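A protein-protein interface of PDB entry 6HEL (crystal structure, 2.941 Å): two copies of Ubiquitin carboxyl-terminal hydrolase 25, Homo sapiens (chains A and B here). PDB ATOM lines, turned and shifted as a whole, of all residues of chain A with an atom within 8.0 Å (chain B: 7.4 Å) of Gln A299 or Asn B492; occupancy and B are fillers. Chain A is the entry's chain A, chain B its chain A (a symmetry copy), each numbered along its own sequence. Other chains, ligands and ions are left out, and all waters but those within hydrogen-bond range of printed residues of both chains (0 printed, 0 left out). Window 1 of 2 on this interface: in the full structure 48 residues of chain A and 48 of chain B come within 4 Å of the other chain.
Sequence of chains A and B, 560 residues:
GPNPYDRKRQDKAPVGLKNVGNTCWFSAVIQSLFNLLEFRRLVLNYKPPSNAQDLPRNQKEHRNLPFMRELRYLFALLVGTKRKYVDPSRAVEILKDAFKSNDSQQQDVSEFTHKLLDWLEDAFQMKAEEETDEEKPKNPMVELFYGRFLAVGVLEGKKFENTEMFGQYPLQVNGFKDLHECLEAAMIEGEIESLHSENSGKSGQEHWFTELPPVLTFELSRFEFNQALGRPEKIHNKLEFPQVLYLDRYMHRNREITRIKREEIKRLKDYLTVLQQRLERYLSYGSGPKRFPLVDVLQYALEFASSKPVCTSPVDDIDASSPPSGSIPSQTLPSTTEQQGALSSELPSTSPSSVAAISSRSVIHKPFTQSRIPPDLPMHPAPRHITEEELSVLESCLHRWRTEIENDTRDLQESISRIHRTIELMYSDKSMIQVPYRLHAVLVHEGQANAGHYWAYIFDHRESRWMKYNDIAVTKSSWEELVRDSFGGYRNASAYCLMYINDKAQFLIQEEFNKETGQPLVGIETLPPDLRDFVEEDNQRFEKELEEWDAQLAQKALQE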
ATOM      1  N   PRO A 293      10.281 -20.768  19.394  1.00  0.00           N
ATOM      2  CA  PRO A 293      10.807 -21.388  20.617  1.00  0.00           C
ATOM      3  C   PRO A 293       9.675 -21.818  21.536  1.00  0.00           C
ATOM      4  O   PRO A 293       8.734 -21.061  21.785  1.00  0.00           O
ATOM      5  CB  PRO A 293      11.655 -20.273  21.240  1.00  0.00           C
ATOM      6  CG  PRO A 293      12.054 -19.422  20.085  1.00  0.00           C
ATOM      7  CD  PRO A 293      10.882 -19.445  19.144  1.00  0.00           C
ATOM      8  N   LEU A 294       9.772 -23.050  22.039  1.00  0.00           N
ATOM      9  CA  LEU A 294       8.667 -23.635  22.794  1.00  0.00           C
ATOM     10  C   LEU A 294       8.427 -22.891  24.103  1.00  0.00           C
ATOM     11  O   LEU A 294       7.275 -22.725  24.529  1.00  0.00           O
ATOM     12  CB  LEU A 294       8.942 -25.118  23.048  1.00  0.00           C
ATOM     13  CG  LEU A 294       7.801 -25.972  23.607  1.00  0.00           C
ATOM     14  CD1 LEU A 294       7.903 -27.391  23.089  1.00  0.00           C
ATOM     15  CD2 LEU A 294       7.817 -25.981  25.123  1.00  0.00           C
ATOM     16  N   VAL A 295       9.499 -22.452  24.766  1.00  0.00           N
ATOM     17  CA  VAL A 295       9.340 -21.657  25.979  1.00  0.00           C
ATOM     18  C   VAL A 295       8.521 -20.406  25.687  1.00  0.00           C
ATOM     19  O   VAL A 295       7.661 -20.003  26.483  1.00  0.00           O
ATOM     20  CB  VAL A 295      10.718 -21.313  26.576  1.00  0.00           C
ATOM     21  CG1 VAL A 295      11.659 -20.800  25.494  1.00  0.00           C
ATOM     22  CG2 VAL A 295      10.575 -20.290  27.683  1.00  0.00           C
ATOM     23  N   ASP A 296       8.757 -19.788  24.527  1.00  0.00           N
ATOM     24  CA  ASP A 296       8.005 -18.596  24.158  1.00  0.00           C
ATOM     25  C   ASP A 296       6.526 -18.910  23.973  1.00  0.00           C
ATOM     26  O   ASP A 296       5.667 -18.153  24.438  1.00  0.00           O
ATOM     27  CB  ASP A 296       8.591 -17.979  22.888  1.00  0.00           C
ATOM     28  CG  ASP A 296       9.938 -17.325  23.127  1.00  0.00           C
ATOM     29  OD1 ASP A 296      10.324 -17.170  24.306  1.00  0.00           O
ATOM     30  OD2 ASP A 296      10.611 -16.970  22.138  1.00  0.00           O
ATOM     31  N   VAL A 297       6.204 -20.023  23.309  1.00  0.00           N
ATOM     32  CA  VAL A 297       4.797 -20.345  23.094  1.00  0.00           C
ATOM     33  C   VAL A 297       4.112 -20.644  24.423  1.00  0.00           C
ATOM     34  O   VAL A 297       2.973 -20.216  24.657  1.00  0.00           O
ATOM     35  CB  VAL A 297       4.641 -21.497  22.075  1.00  0.00           C
ATOM     36  CG1 VAL A 297       5.621 -21.327  20.924  1.00  0.00           C
ATOM     37  CG2 VAL A 297       4.793 -22.873  22.717  1.00  0.00           C
ATOM     38  N   LEU A 298       4.811 -21.321  25.339  1.00  0.00           N
ATOM     39  CA  LEU A 298       4.215 -21.618  26.638  1.00  0.00           C
ATOM     40  C   LEU A 298       3.958 -20.342  27.428  1.00  0.00           C
ATOM     41  O   LEU A 298       2.855 -20.136  27.953  1.00  0.00           O
ATOM     42  CB  LEU A 298       5.111 -22.569  27.429  1.00  0.00           C
ATOM     43  CG  LEU A 298       5.167 -24.008  26.920  1.00  0.00           C
ATOM     44  CD1 LEU A 298       5.889 -24.890  27.922  1.00  0.00           C
ATOM     45  CD2 LEU A 298       3.769 -24.541  26.639  1.00  0.00           C
ATOM     46  N   GLN A 299       4.966 -19.471  27.521  1.00  0.00           N
ATOM     47  CA  GLN A 299       4.807 -18.231  28.272  1.00  0.00           C
ATOM     48  C   GLN A 299       3.712 -17.358  27.671  1.00  0.00           C
ATOM     49  O   GLN A 299       2.884 -16.788  28.397  1.00  0.00           O
ATOM     50  CB  GLN A 299       6.131 -17.471  28.311  1.00  0.00           C
ATOM     51  CG  GLN A 299       5.998 -16.051  28.821  1.00  0.00           C
ATOM     52  CD  GLN A 299       7.212 -15.209  28.512  1.00  0.00           C
ATOM     53  OE1 GLN A 299       8.182 -15.688  27.922  1.00  0.00           O
ATOM     54  NE2 GLN A 299       7.166 -13.942  28.902  1.00  0.00           N
ATOM     55  N   TYR A 300       3.694 -17.237  26.341  1.00  0.00           N
ATOM     56  CA  TYR A 300       2.695 -16.403  25.684  1.00  0.00           C
ATOM     57  C   TYR A 300       1.290 -16.935  25.927  1.00  0.00           C
ATOM     58  O   TYR A 300       0.378 -16.173  26.266  1.00  0.00           O
ATOM     59  CB  TYR A 300       2.993 -16.318  24.186  1.00  0.00           C
ATOM     60  CG  TYR A 300       4.219 -15.499  23.849  1.00  0.00           C
ATOM     61  CD1 TYR A 300       4.699 -14.541  24.727  1.00  0.00           C
ATOM     62  CD2 TYR A 300       4.891 -15.680  22.650  1.00  0.00           C
ATOM     63  CE1 TYR A 300       5.820 -13.792  24.423  1.00  0.00           C
ATOM     64  CE2 TYR A 300       6.011 -14.933  22.338  1.00  0.00           C
ATOM     65  CZ  TYR A 300       6.469 -13.988  23.227  1.00  0.00           C
ATOM     66  OH  TYR A 300       7.583 -13.238  22.926  1.00  0.00           O
ATOM     67  N   ALA A 301       1.095 -18.248  25.770  1.00  0.00           N
ATOM     68  CA  ALA A 301      -0.226 -18.821  26.001  1.00  0.00           C
ATOM     69  C   ALA A 301      -0.663 -18.639  27.450  1.00  0.00           C
ATOM     70  O   ALA A 301      -1.820 -18.281  27.718  1.00  0.00           O
ATOM     71  CB  ALA A 301      -0.228 -20.300  25.619  1.00  0.00           C
ATOM     72  N   LEU A 302       0.247 -18.875  28.399  1.00  0.00           N
ATOM     73  CA  LEU A 302      -0.095 -18.703  29.807  1.00  0.00           C
ATOM     74  C   LEU A 302      -0.529 -17.274  30.095  1.00  0.00           C
ATOM     75  O   LEU A 302      -1.586 -17.041  30.693  1.00  0.00           O
ATOM     76  CB  LEU A 302       1.088 -19.094  30.690  1.00  0.00           C
ATOM     77  CG  LEU A 302       0.974 -18.720  32.169  1.00  0.00           C
ATOM     78  CD1 LEU A 302      -0.323 -19.229  32.783  1.00  0.00           C
ATOM     79  CD2 LEU A 302       2.166 -19.273  32.919  1.00  0.00           C
ATOM     80  N   GLU A 303       0.275 -16.296  29.679  1.00  0.00           N
ATOM     81  CA  GLU A 303      -0.096 -14.915  29.951  1.00  0.00           C
ATOM     82  C   GLU A 303      -1.319 -14.476  29.157  1.00  0.00           C
ATOM     83  O   GLU A 303      -1.940 -13.468  29.508  1.00  0.00           O
ATOM     84  CB  GLU A 303       1.061 -13.987  29.641  1.00  0.00           C
ATOM     85  CG  GLU A 303       1.229 -13.746  28.176  1.00  0.00           C
ATOM     86  CD  GLU A 303       2.363 -12.818  27.919  1.00  0.00           C
ATOM     87  OE1 GLU A 303       2.165 -11.813  27.209  1.00  0.00           O
ATOM     88  OE2 GLU A 303       3.457 -13.080  28.465  1.00  0.00           O
ATOM     89  N   PHE A 304      -1.658 -15.187  28.081  1.00  0.00           N
ATOM     90  CA  PHE A 304      -2.931 -14.932  27.421  1.00  0.00           C
ATOM     91  C   PHE A 304      -4.088 -15.410  28.280  1.00  0.00           C
ATOM     92  O   PHE A 304      -5.107 -14.720  28.400  1.00  0.00           O
ATOM     93  CB  PHE A 304      -2.967 -15.610  26.054  1.00  0.00           C
ATOM     94  CG  PHE A 304      -4.357 -15.869  25.546  1.00  0.00           C
ATOM     95  CD1 PHE A 304      -5.115 -14.846  25.007  1.00  0.00           C
ATOM     96  CD2 PHE A 304      -4.905 -17.140  25.610  1.00  0.00           C
ATOM     97  CE1 PHE A 304      -6.393 -15.084  24.539  1.00  0.00           C
ATOM     98  CE2 PHE A 304      -6.183 -17.380  25.145  1.00  0.00           C
ATOM     99  CZ  PHE A 304      -6.927 -16.351  24.609  1.00  0.00           C
ATOM    100  N   ALA A 305      -3.950 -16.593  28.881  1.00  0.00           N
ATOM    101  CA  ALA A 305      -5.004 -17.091  29.759  1.00  0.00           C
ATOM    102  C   ALA A 305      -5.147 -16.214  30.998  1.00  0.00           C
ATOM    103  O   ALA A 305      -6.257 -16.029  31.514  1.00  0.00           O
ATOM    104  CB  ALA A 305      -4.722 -18.539  30.151  1.00  0.00           C
ATOM    105  N   SER A 306      -4.035 -15.657  31.485  1.00  0.00           N
ATOM    106  CA  SER A 306      -4.082 -14.826  32.685  1.00  0.00           C
ATOM    107  C   SER A 306      -4.849 -13.531  32.447  1.00  0.00           C
ATOM    108  O   SER A 306      -5.415 -12.964  33.388  1.00  0.00           O
ATOM    109  CB  SER A 306      -2.663 -14.511  33.157  1.00  0.00           C
ATOM    110  OG  SER A 306      -1.849 -15.670  33.137  1.00  0.00           O
ATOM    111  N   LEU A 398       1.414 -24.967  32.991  1.00  0.00           N
ATOM    112  CA  LEU A 398       2.247 -24.194  32.082  1.00  0.00           C
ATOM    113  C   LEU A 398       3.511 -23.688  32.767  1.00  0.00           C
ATOM    114  O   LEU A 398       4.586 -23.696  32.160  1.00  0.00           O
ATOM    115  CB  LEU A 398       1.445 -23.039  31.488  1.00  0.00           C
ATOM    116  CG  LEU A 398       0.480 -23.501  30.394  1.00  0.00           C
ATOM    117  CD1 LEU A 398      -0.135 -22.321  29.667  1.00  0.00           C
ATOM    118  CD2 LEU A 398       1.192 -24.421  29.413  1.00  0.00           C
ATOM    119  N   HIS A 399       3.419 -23.258  34.029  1.00  0.00           N
ATOM    120  CA  HIS A 399       4.613 -22.804  34.735  1.00  0.00           C
ATOM    121  C   HIS A 399       5.608 -23.945  34.924  1.00  0.00           C
ATOM    122  O   HIS A 399       6.809 -23.781  34.659  1.00  0.00           O
ATOM    123  CB  HIS A 399       4.231 -22.194  36.084  1.00  0.00           C
ATOM    124  CG  HIS A 399       3.988 -20.718  36.035  1.00  0.00           C
ATOM    125  ND1 HIS A 399       5.000 -19.804  35.834  1.00  0.00           N
ATOM    126  CD2 HIS A 399       2.851 -19.996  36.171  1.00  0.00           C
ATOM    127  CE1 HIS A 399       4.495 -18.582  35.842  1.00  0.00           C
ATOM    128  NE2 HIS A 399       3.193 -18.672  36.045  1.00  0.00           N
ATOM    129  N   ARG A 402       7.166 -24.795  31.545  1.00  0.00           N
ATOM    130  CA  ARG A 402       8.125 -23.796  31.096  1.00  0.00           C
ATOM    131  C   ARG A 402       9.435 -23.912  31.864  1.00  0.00           C
ATOM    132  O   ARG A 402      10.519 -23.814  31.273  1.00  0.00           O
ATOM    133  CB  ARG A 402       7.522 -22.400  31.242  1.00  0.00           C
ATOM    134  CG  ARG A 402       8.533 -21.294  31.437  1.00  0.00           C
ATOM    135  CD  ARG A 402       8.098 -20.021  30.731  1.00  0.00           C
ATOM    136  NE  ARG A 402       8.598 -18.834  31.415  1.00  0.00           N
ATOM    137  CZ  ARG A 402       9.853 -18.403  31.352  1.00  0.00           C
ATOM    138  NH1 ARG A 402      10.213 -17.317  32.016  1.00  0.00           N
ATOM    139  NH2 ARG A 402      10.752 -19.059  30.634  1.00  0.00           N
ATOM    140  N   GLU A 406      13.051 -24.809  30.198  1.00  0.00           N
ATOM    141  CA  GLU A 406      14.236 -23.986  30.424  1.00  0.00           C
ATOM    142  C   GLU A 406      15.407 -24.839  30.894  1.00  0.00           C
ATOM    143  O   GLU A 406      16.530 -24.715  30.383  1.00  0.00           O
ATOM    144  CB  GLU A 406      13.940 -22.889  31.448  1.00  0.00           C
ATOM    145  CG  GLU A 406      13.060 -21.763  30.945  1.00  0.00           C
ATOM    146  CD  GLU A 406      13.200 -20.510  31.788  1.00  0.00           C
ATOM    147  OE1 GLU A 406      13.389 -19.419  31.210  1.00  0.00           O
ATOM    148  OE2 GLU A 406      13.134 -20.617  33.031  1.00  0.00           O
ATOM    149  N   LYS B 234       6.131  -2.700  26.124  1.00  0.00           N
ATOM    150  CA  LYS B 234       7.473  -2.558  26.677  1.00  0.00           C
ATOM    151  C   LYS B 234       8.469  -2.640  25.525  1.00  0.00           C
ATOM    152  O   LYS B 234       8.713  -3.723  24.985  1.00  0.00           O
ATOM    153  CB  LYS B 234       7.748  -3.635  27.723  1.00  0.00           C
ATOM    154  N   HIS B 236      11.796  -3.038  23.557  1.00  0.00           N
ATOM    155  CA  HIS B 236      12.874  -3.973  23.859  1.00  0.00           C
ATOM    156  C   HIS B 236      14.204  -3.540  23.251  1.00  0.00           C
ATOM    157  O   HIS B 236      14.972  -4.363  22.748  1.00  0.00           O
ATOM    158  CB  HIS B 236      12.513  -5.380  23.391  1.00  0.00           C
ATOM    159  CG  HIS B 236      11.368  -5.988  24.137  1.00  0.00           C
ATOM    160  ND1 HIS B 236      10.075  -5.963  23.664  1.00  0.00           N
ATOM    161  CD2 HIS B 236      11.323  -6.637  25.324  1.00  0.00           C
ATOM    162  CE1 HIS B 236       9.282  -6.573  24.525  1.00  0.00           C
ATOM    163  NE2 HIS B 236      10.013  -6.992  25.542  1.00  0.00           N
ATOM    164  N   HIS B 445      12.483  -7.877  35.213  1.00  0.00           N
ATOM    165  CA  HIS B 445      11.085  -8.213  34.984  1.00  0.00           C
ATOM    166  C   HIS B 445      10.946  -8.992  33.681  1.00  0.00           C
ATOM    167  O   HIS B 445      11.760  -8.847  32.765  1.00  0.00           O
ATOM    168  CB  HIS B 445      10.230  -6.932  34.936  1.00  0.00           C
ATOM    169  CG  HIS B 445       8.825  -7.145  34.464  1.00  0.00           C
ATOM    170  ND1 HIS B 445       7.766  -7.306  35.330  1.00  0.00           N
ATOM    171  CD2 HIS B 445       8.303  -7.211  33.216  1.00  0.00           C
ATOM    172  CE1 HIS B 445       6.652  -7.468  34.637  1.00  0.00           C
ATOM    173  NE2 HIS B 445       6.952  -7.417  33.351  1.00  0.00           N
ATOM    174  N   GLU B 446       9.902  -9.817  33.604  1.00  0.00           N
ATOM    175  CA  GLU B 446       9.667 -10.647  32.422  1.00  0.00           C
ATOM    176  C   GLU B 446       8.174 -10.892  32.263  1.00  0.00           C
ATOM    177  O   GLU B 446       7.584 -11.646  33.040  1.00  0.00           O
ATOM    178  CB  GLU B 446      10.418 -11.969  32.531  1.00  0.00           C
ATOM    179  CG  GLU B 446      10.024 -12.985  31.476  1.00  0.00           C
ATOM    180  CD  GLU B 446      10.513 -14.377  31.802  1.00  0.00           C
ATOM    181  OE1 GLU B 446      10.191 -14.882  32.898  1.00  0.00           O
ATOM    182  OE2 GLU B 446      11.225 -14.970  30.966  1.00  0.00           O
ATOM    183  N   GLY B 447       7.567 -10.283  31.245  1.00  0.00           N
ATOM    184  CA  GLY B 447       6.180 -10.534  30.932  1.00  0.00           C
ATOM    185  C   GLY B 447       5.424  -9.238  30.767  1.00  0.00           C
ATOM    186  O   GLY B 447       6.016  -8.173  30.559  1.00  0.00           O
ATOM    187  N   GLN B 448       4.100  -9.334  30.858  1.00  0.00           N
ATOM    188  CA  GLN B 448       3.260  -8.154  30.742  1.00  0.00           C
ATOM    189  C   GLN B 448       3.491  -7.216  31.922  1.00  0.00           C
ATOM    190  O   GLN B 448       3.942  -7.619  32.999  1.00  0.00           O
ATOM    191  CB  GLN B 448       1.786  -8.549  30.653  1.00  0.00           C
ATOM    192  CG  GLN B 448       1.236  -8.513  29.238  1.00  0.00           C
ATOM    193  CD  GLN B 448       0.224  -9.607  28.978  1.00  0.00           C
ATOM    194  OE1 GLN B 448      -0.510 -10.018  29.875  1.00  0.00           O
ATOM    195  NE2 GLN B 448       0.189 -10.097  27.743  1.00  0.00           N
ATOM    196  N   GLY B 452       3.727 -10.006  35.602  1.00  0.00           N
ATOM    197  CA  GLY B 452       4.948 -10.567  35.070  1.00  0.00           C
ATOM    198  C   GLY B 452       5.747 -11.201  36.186  1.00  0.00           C
ATOM    199  O   GLY B 452       5.356 -11.172  37.354  1.00  0.00           O
ATOM    200  N   HIS B 453       6.877 -11.786  35.811  1.00  0.00           N
ATOM    201  CA  HIS B 453       7.788 -12.411  36.754  1.00  0.00           C
ATOM    202  C   HIS B 453       8.896 -11.436  37.126  1.00  0.00           C
ATOM    203  O   HIS B 453       9.301 -10.594  36.321  1.00  0.00           O
ATOM    204  CB  HIS B 453       8.393 -13.689  36.170  1.00  0.00           C
ATOM    205  CG  HIS B 453       8.900 -14.641  37.206  1.00  0.00           C
ATOM    206  ND1 HIS B 453      10.130 -14.503  37.810  1.00  0.00           N
ATOM    207  CD2 HIS B 453       8.336 -15.746  37.749  1.00  0.00           C
ATOM    208  CE1 HIS B 453      10.305 -15.483  38.679  1.00  0.00           C
ATOM    209  NE2 HIS B 453       9.231 -16.251  38.661  1.00  0.00           N
ATOM    210  N   TRP B 455      12.782 -11.057  39.227  1.00  0.00           N
ATOM    211  CA  TRP B 455      13.900 -11.600  39.992  1.00  0.00           C
ATOM    212  C   TRP B 455      14.994 -10.543  40.042  1.00  0.00           C
ATOM    213  O   TRP B 455      14.861  -9.463  39.463  1.00  0.00           O
ATOM    214  CB  TRP B 455      14.396 -12.938  39.422  1.00  0.00           C
ATOM    215  CG  TRP B 455      14.963 -12.915  38.036  1.00  0.00           C
ATOM    216  CD1 TRP B 455      16.276 -12.772  37.693  1.00  0.00           C
ATOM    217  CD2 TRP B 455      14.244 -13.087  36.806  1.00  0.00           C
ATOM    218  NE1 TRP B 455      16.418 -12.827  36.327  1.00  0.00           N
ATOM    219  CE2 TRP B 455      15.186 -13.022  35.759  1.00  0.00           C
ATOM    220  CE3 TRP B 455      12.896 -13.283  36.488  1.00  0.00           C
ATOM    221  CZ2 TRP B 455      14.823 -13.135  34.418  1.00  0.00           C
ATOM    222  CZ3 TRP B 455      12.538 -13.401  35.153  1.00  0.00           C
ATOM    223  CH2 TRP B 455      13.499 -13.327  34.137  1.00  0.00           C
ATOM    224  N   ARG B 484      22.864 -10.768  29.968  1.00  0.00           N
ATOM    225  CA  ARG B 484      21.905 -11.562  29.212  1.00  0.00           C
ATOM    226  C   ARG B 484      20.475 -11.304  29.670  1.00  0.00           C
ATOM    227  O   ARG B 484      19.542 -11.410  28.866  1.00  0.00           O
ATOM    228  CB  ARG B 484      22.237 -13.048  29.348  1.00  0.00           C
ATOM    229  CG  ARG B 484      22.242 -13.817  28.040  1.00  0.00           C
ATOM    230  CD  ARG B 484      21.853 -15.266  28.277  1.00  0.00           C
ATOM    231  NE  ARG B 484      20.460 -15.365  28.699  1.00  0.00           N
ATOM    232  CZ  ARG B 484      19.451 -15.625  27.875  1.00  0.00           C
ATOM    233  NH1 ARG B 484      18.211 -15.689  28.341  1.00  0.00           N
ATOM    234  NH2 ARG B 484      19.685 -15.831  26.586  1.00  0.00           N
ATOM    235  N   ASP B 485      20.263 -11.021  30.943  1.00  0.00           N
ATOM    236  CA  ASP B 485      18.900 -10.770  31.390  1.00  0.00           C
ATOM    237  C   ASP B 485      18.575  -9.290  31.527  1.00  0.00           C
ATOM    238  O   ASP B 485      17.525  -8.834  31.095  1.00  0.00           O
ATOM    239  CB  ASP B 485      18.616 -11.496  32.707  1.00  0.00           C
ATOM    240  CG  ASP B 485      18.737 -13.002  32.583  1.00  0.00           C
ATOM    241  OD1 ASP B 485      19.602 -13.587  33.256  1.00  0.00           O
ATOM    242  OD2 ASP B 485      17.967 -13.605  31.815  1.00  0.00           O
ATOM    243  N   GLY B 488      18.340  -6.446  27.898  1.00  0.00           N
ATOM    244  CA  GLY B 488      17.188  -6.404  27.022  1.00  0.00           C
ATOM    245  C   GLY B 488      17.596  -6.687  25.593  1.00  0.00           C
ATOM    246  O   GLY B 488      18.730  -6.460  25.201  1.00  0.00           O
ATOM    247  N   GLY B 489      16.649  -7.160  24.800  1.00  0.00           N
ATOM    248  CA  GLY B 489      16.917  -7.530  23.427  1.00  0.00           C
ATOM    249  C   GLY B 489      17.331  -8.987  23.483  1.00  0.00           C
ATOM    250  O   GLY B 489      17.434  -9.672  22.471  1.00  0.00           O
ATOM    251  N   TYR B 490      17.543  -9.458  24.706  1.00  0.00           N
ATOM    252  CA  TYR B 490      17.882 -10.851  24.977  1.00  0.00           C
ATOM    253  C   TYR B 490      16.694 -11.496  25.678  1.00  0.00           C
ATOM    254  O   TYR B 490      16.363 -11.128  26.810  1.00  0.00           O
ATOM    255  CB  TYR B 490      19.144 -10.967  25.830  1.00  0.00           C
ATOM    256  CG  TYR B 490      20.362 -10.256  25.283  1.00  0.00           C
ATOM    257  CD1 TYR B 490      21.398  -9.878  26.126  1.00  0.00           C
ATOM    258  CD2 TYR B 490      20.483  -9.969  23.931  1.00  0.00           C
ATOM    259  CE1 TYR B 490      22.514  -9.230  25.640  1.00  0.00           C
ATOM    260  CE2 TYR B 490      21.597  -9.318  23.436  1.00  0.00           C
ATOM    261  CZ  TYR B 490      22.609  -8.953  24.296  1.00  0.00           C
ATOM    262  OH  TYR B 490      23.723  -8.306  23.813  1.00  0.00           O
ATOM    263  N   ARG B 491      16.054 -12.445  25.005  1.00  0.00           N
ATOM    264  CA  ARG B 491      14.862 -13.145  25.519  1.00  0.00           C
ATOM    265  C   ARG B 491      13.809 -12.078  25.841  1.00  0.00           C
ATOM    266  O   ARG B 491      13.760 -11.038  25.167  1.00  0.00           O
ATOM    267  CB  ARG B 491      15.249 -14.039  26.683  1.00  0.00           C
ATOM    268  N   ASN B 492      12.969 -12.291  26.850  1.00  0.00           N
ATOM    269  CA  ASN B 492      11.983 -11.305  27.270  1.00  0.00           C
ATOM    270  C   ASN B 492      12.459 -10.483  28.454  1.00  0.00           C
ATOM    271  O   ASN B 492      11.680  -9.712  29.023  1.00  0.00           O
ATOM    272  CB  ASN B 492      10.664 -11.997  27.606  1.00  0.00           C
ATOM    273  CG  ASN B 492      10.245 -12.981  26.539  1.00  0.00           C
ATOM    274  OD1 ASN B 492      10.744 -12.937  25.416  1.00  0.00           O
ATOM    275  ND2 ASN B 492       9.334 -13.878  26.883  1.00  0.00           N
ATOM    276  N   ALA B 493      13.725 -10.623  28.827  1.00  0.00           N
ATOM    277  CA  ALA B 493      14.214 -10.025  30.055  1.00  0.00           C
ATOM    278  C   ALA B 493      14.412  -8.522  29.897  1.00  0.00           C
ATOM    279  O   ALA B 493      14.824  -8.034  28.840  1.00  0.00           O
ATOM    280  CB  ALA B 493      15.520 -10.696  30.464  1.00  0.00           C
ATOM    281  N   SER B 494      14.101  -7.789  30.961  1.00  0.00           N
ATOM    282  CA  SER B 494      14.307  -6.352  31.029  1.00  0.00           C
ATOM    283  C   SER B 494      14.803  -6.010  32.423  1.00  0.00           C
ATOM    284  O   SER B 494      14.500  -6.714  33.386  1.00  0.00           O
ATOM    285  CB  SER B 494      13.017  -5.579  30.727  1.00  0.00           C
ATOM    286  OG  SER B 494      12.252  -6.232  29.730  1.00  0.00           O
ATOM    287  N   ALA B 495      15.567  -4.929  32.528  1.00  0.00           N
ATOM    288  CA  ALA B 495      16.053  -4.437  33.813  1.00  0.00           C
ATOM    289  C   ALA B 495      15.241  -3.202  34.176  1.00  0.00           C
ATOM    290  O   ALA B 495      15.356  -2.163  33.518  1.00  0.00           O
ATOM    291  CB  ALA B 495      17.543  -4.115  33.755  1.00  0.00           C
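No position is printed for both chains.
Among the printed residues, pairs that only touch across the chains: Gln A299 with Glu B446.
Pro A293 touches none of the printed residues of chain B. Printed residues of chain B within 4 Å of Gln A299: Glu B446 and Asn B492. Of the printed residues of chain B, Glu A303 touches Gln B448 (2.7 Å). Of the printed residues of chain B, Arg A402 touches Glu B446. Of the printed residues of chain A, Glu B446 touches Gln A299 (3.96 Å) and Arg A402 (2.6 Å). Printed residues of chain A within 4 Å of Gln B448: Glu A303 (2.7 Å). No residue of chain A comes within 4 Å of Arg B491. Asn B492 touches just one residue of chain A: Gln A299. Ala B493 touches none of the printed residues of chain A. The nearest residue of chain A that does not touch Asn B492 is Tyr A300 (4.04 Å).
The side-chain amide nitrogen (NE2) of Gln A299 sits close to the side-chain amide nitrogen (ND2) of Asn B492, at 3.0 Å. The side-chain carboxylate of Glu A303 sits at hydrogen-bond distance from the side-chain amide nitrogen of Gln B448, 2.7 Å away. The guanidinium group of Arg A402 is in salt-bridge range of the side-chain carboxylate of Glu B446 (2.6 Å).
The guanidinium group (NH2) of Arg A402 is in salt-bridge range of the side-chain carboxylate (OE1) of Glu A406 (2.7 Å). O of Gln B448 lies within hydrogen-bond range of NE2 of His B445 (3.0 Å). The backbone NH of His B453 lies within hydrogen-bond range of the backbone carbonyl oxygen of Glu B446, 2.9 Å away.
Printed residues of chain B that touch a printed residue of chain A: Glu B446, Gln B448 and Asn B492. Of the 18 printed residues of chain A, 3 touch a printed residue of chain B. Printed residues of chain A that touch a printed residue of chain B: Gln A299, Glu A303 and Arg A402. Along chain A the printed residues that touch a printed residue of chain B span positions 299 to 402. Among the printed residues, Asp or Glu carboxylates within 4 Å of a Lys or Arg side-chain nitrogen of the other chain: Arg A402 with Glu B446 (2.6 Å).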
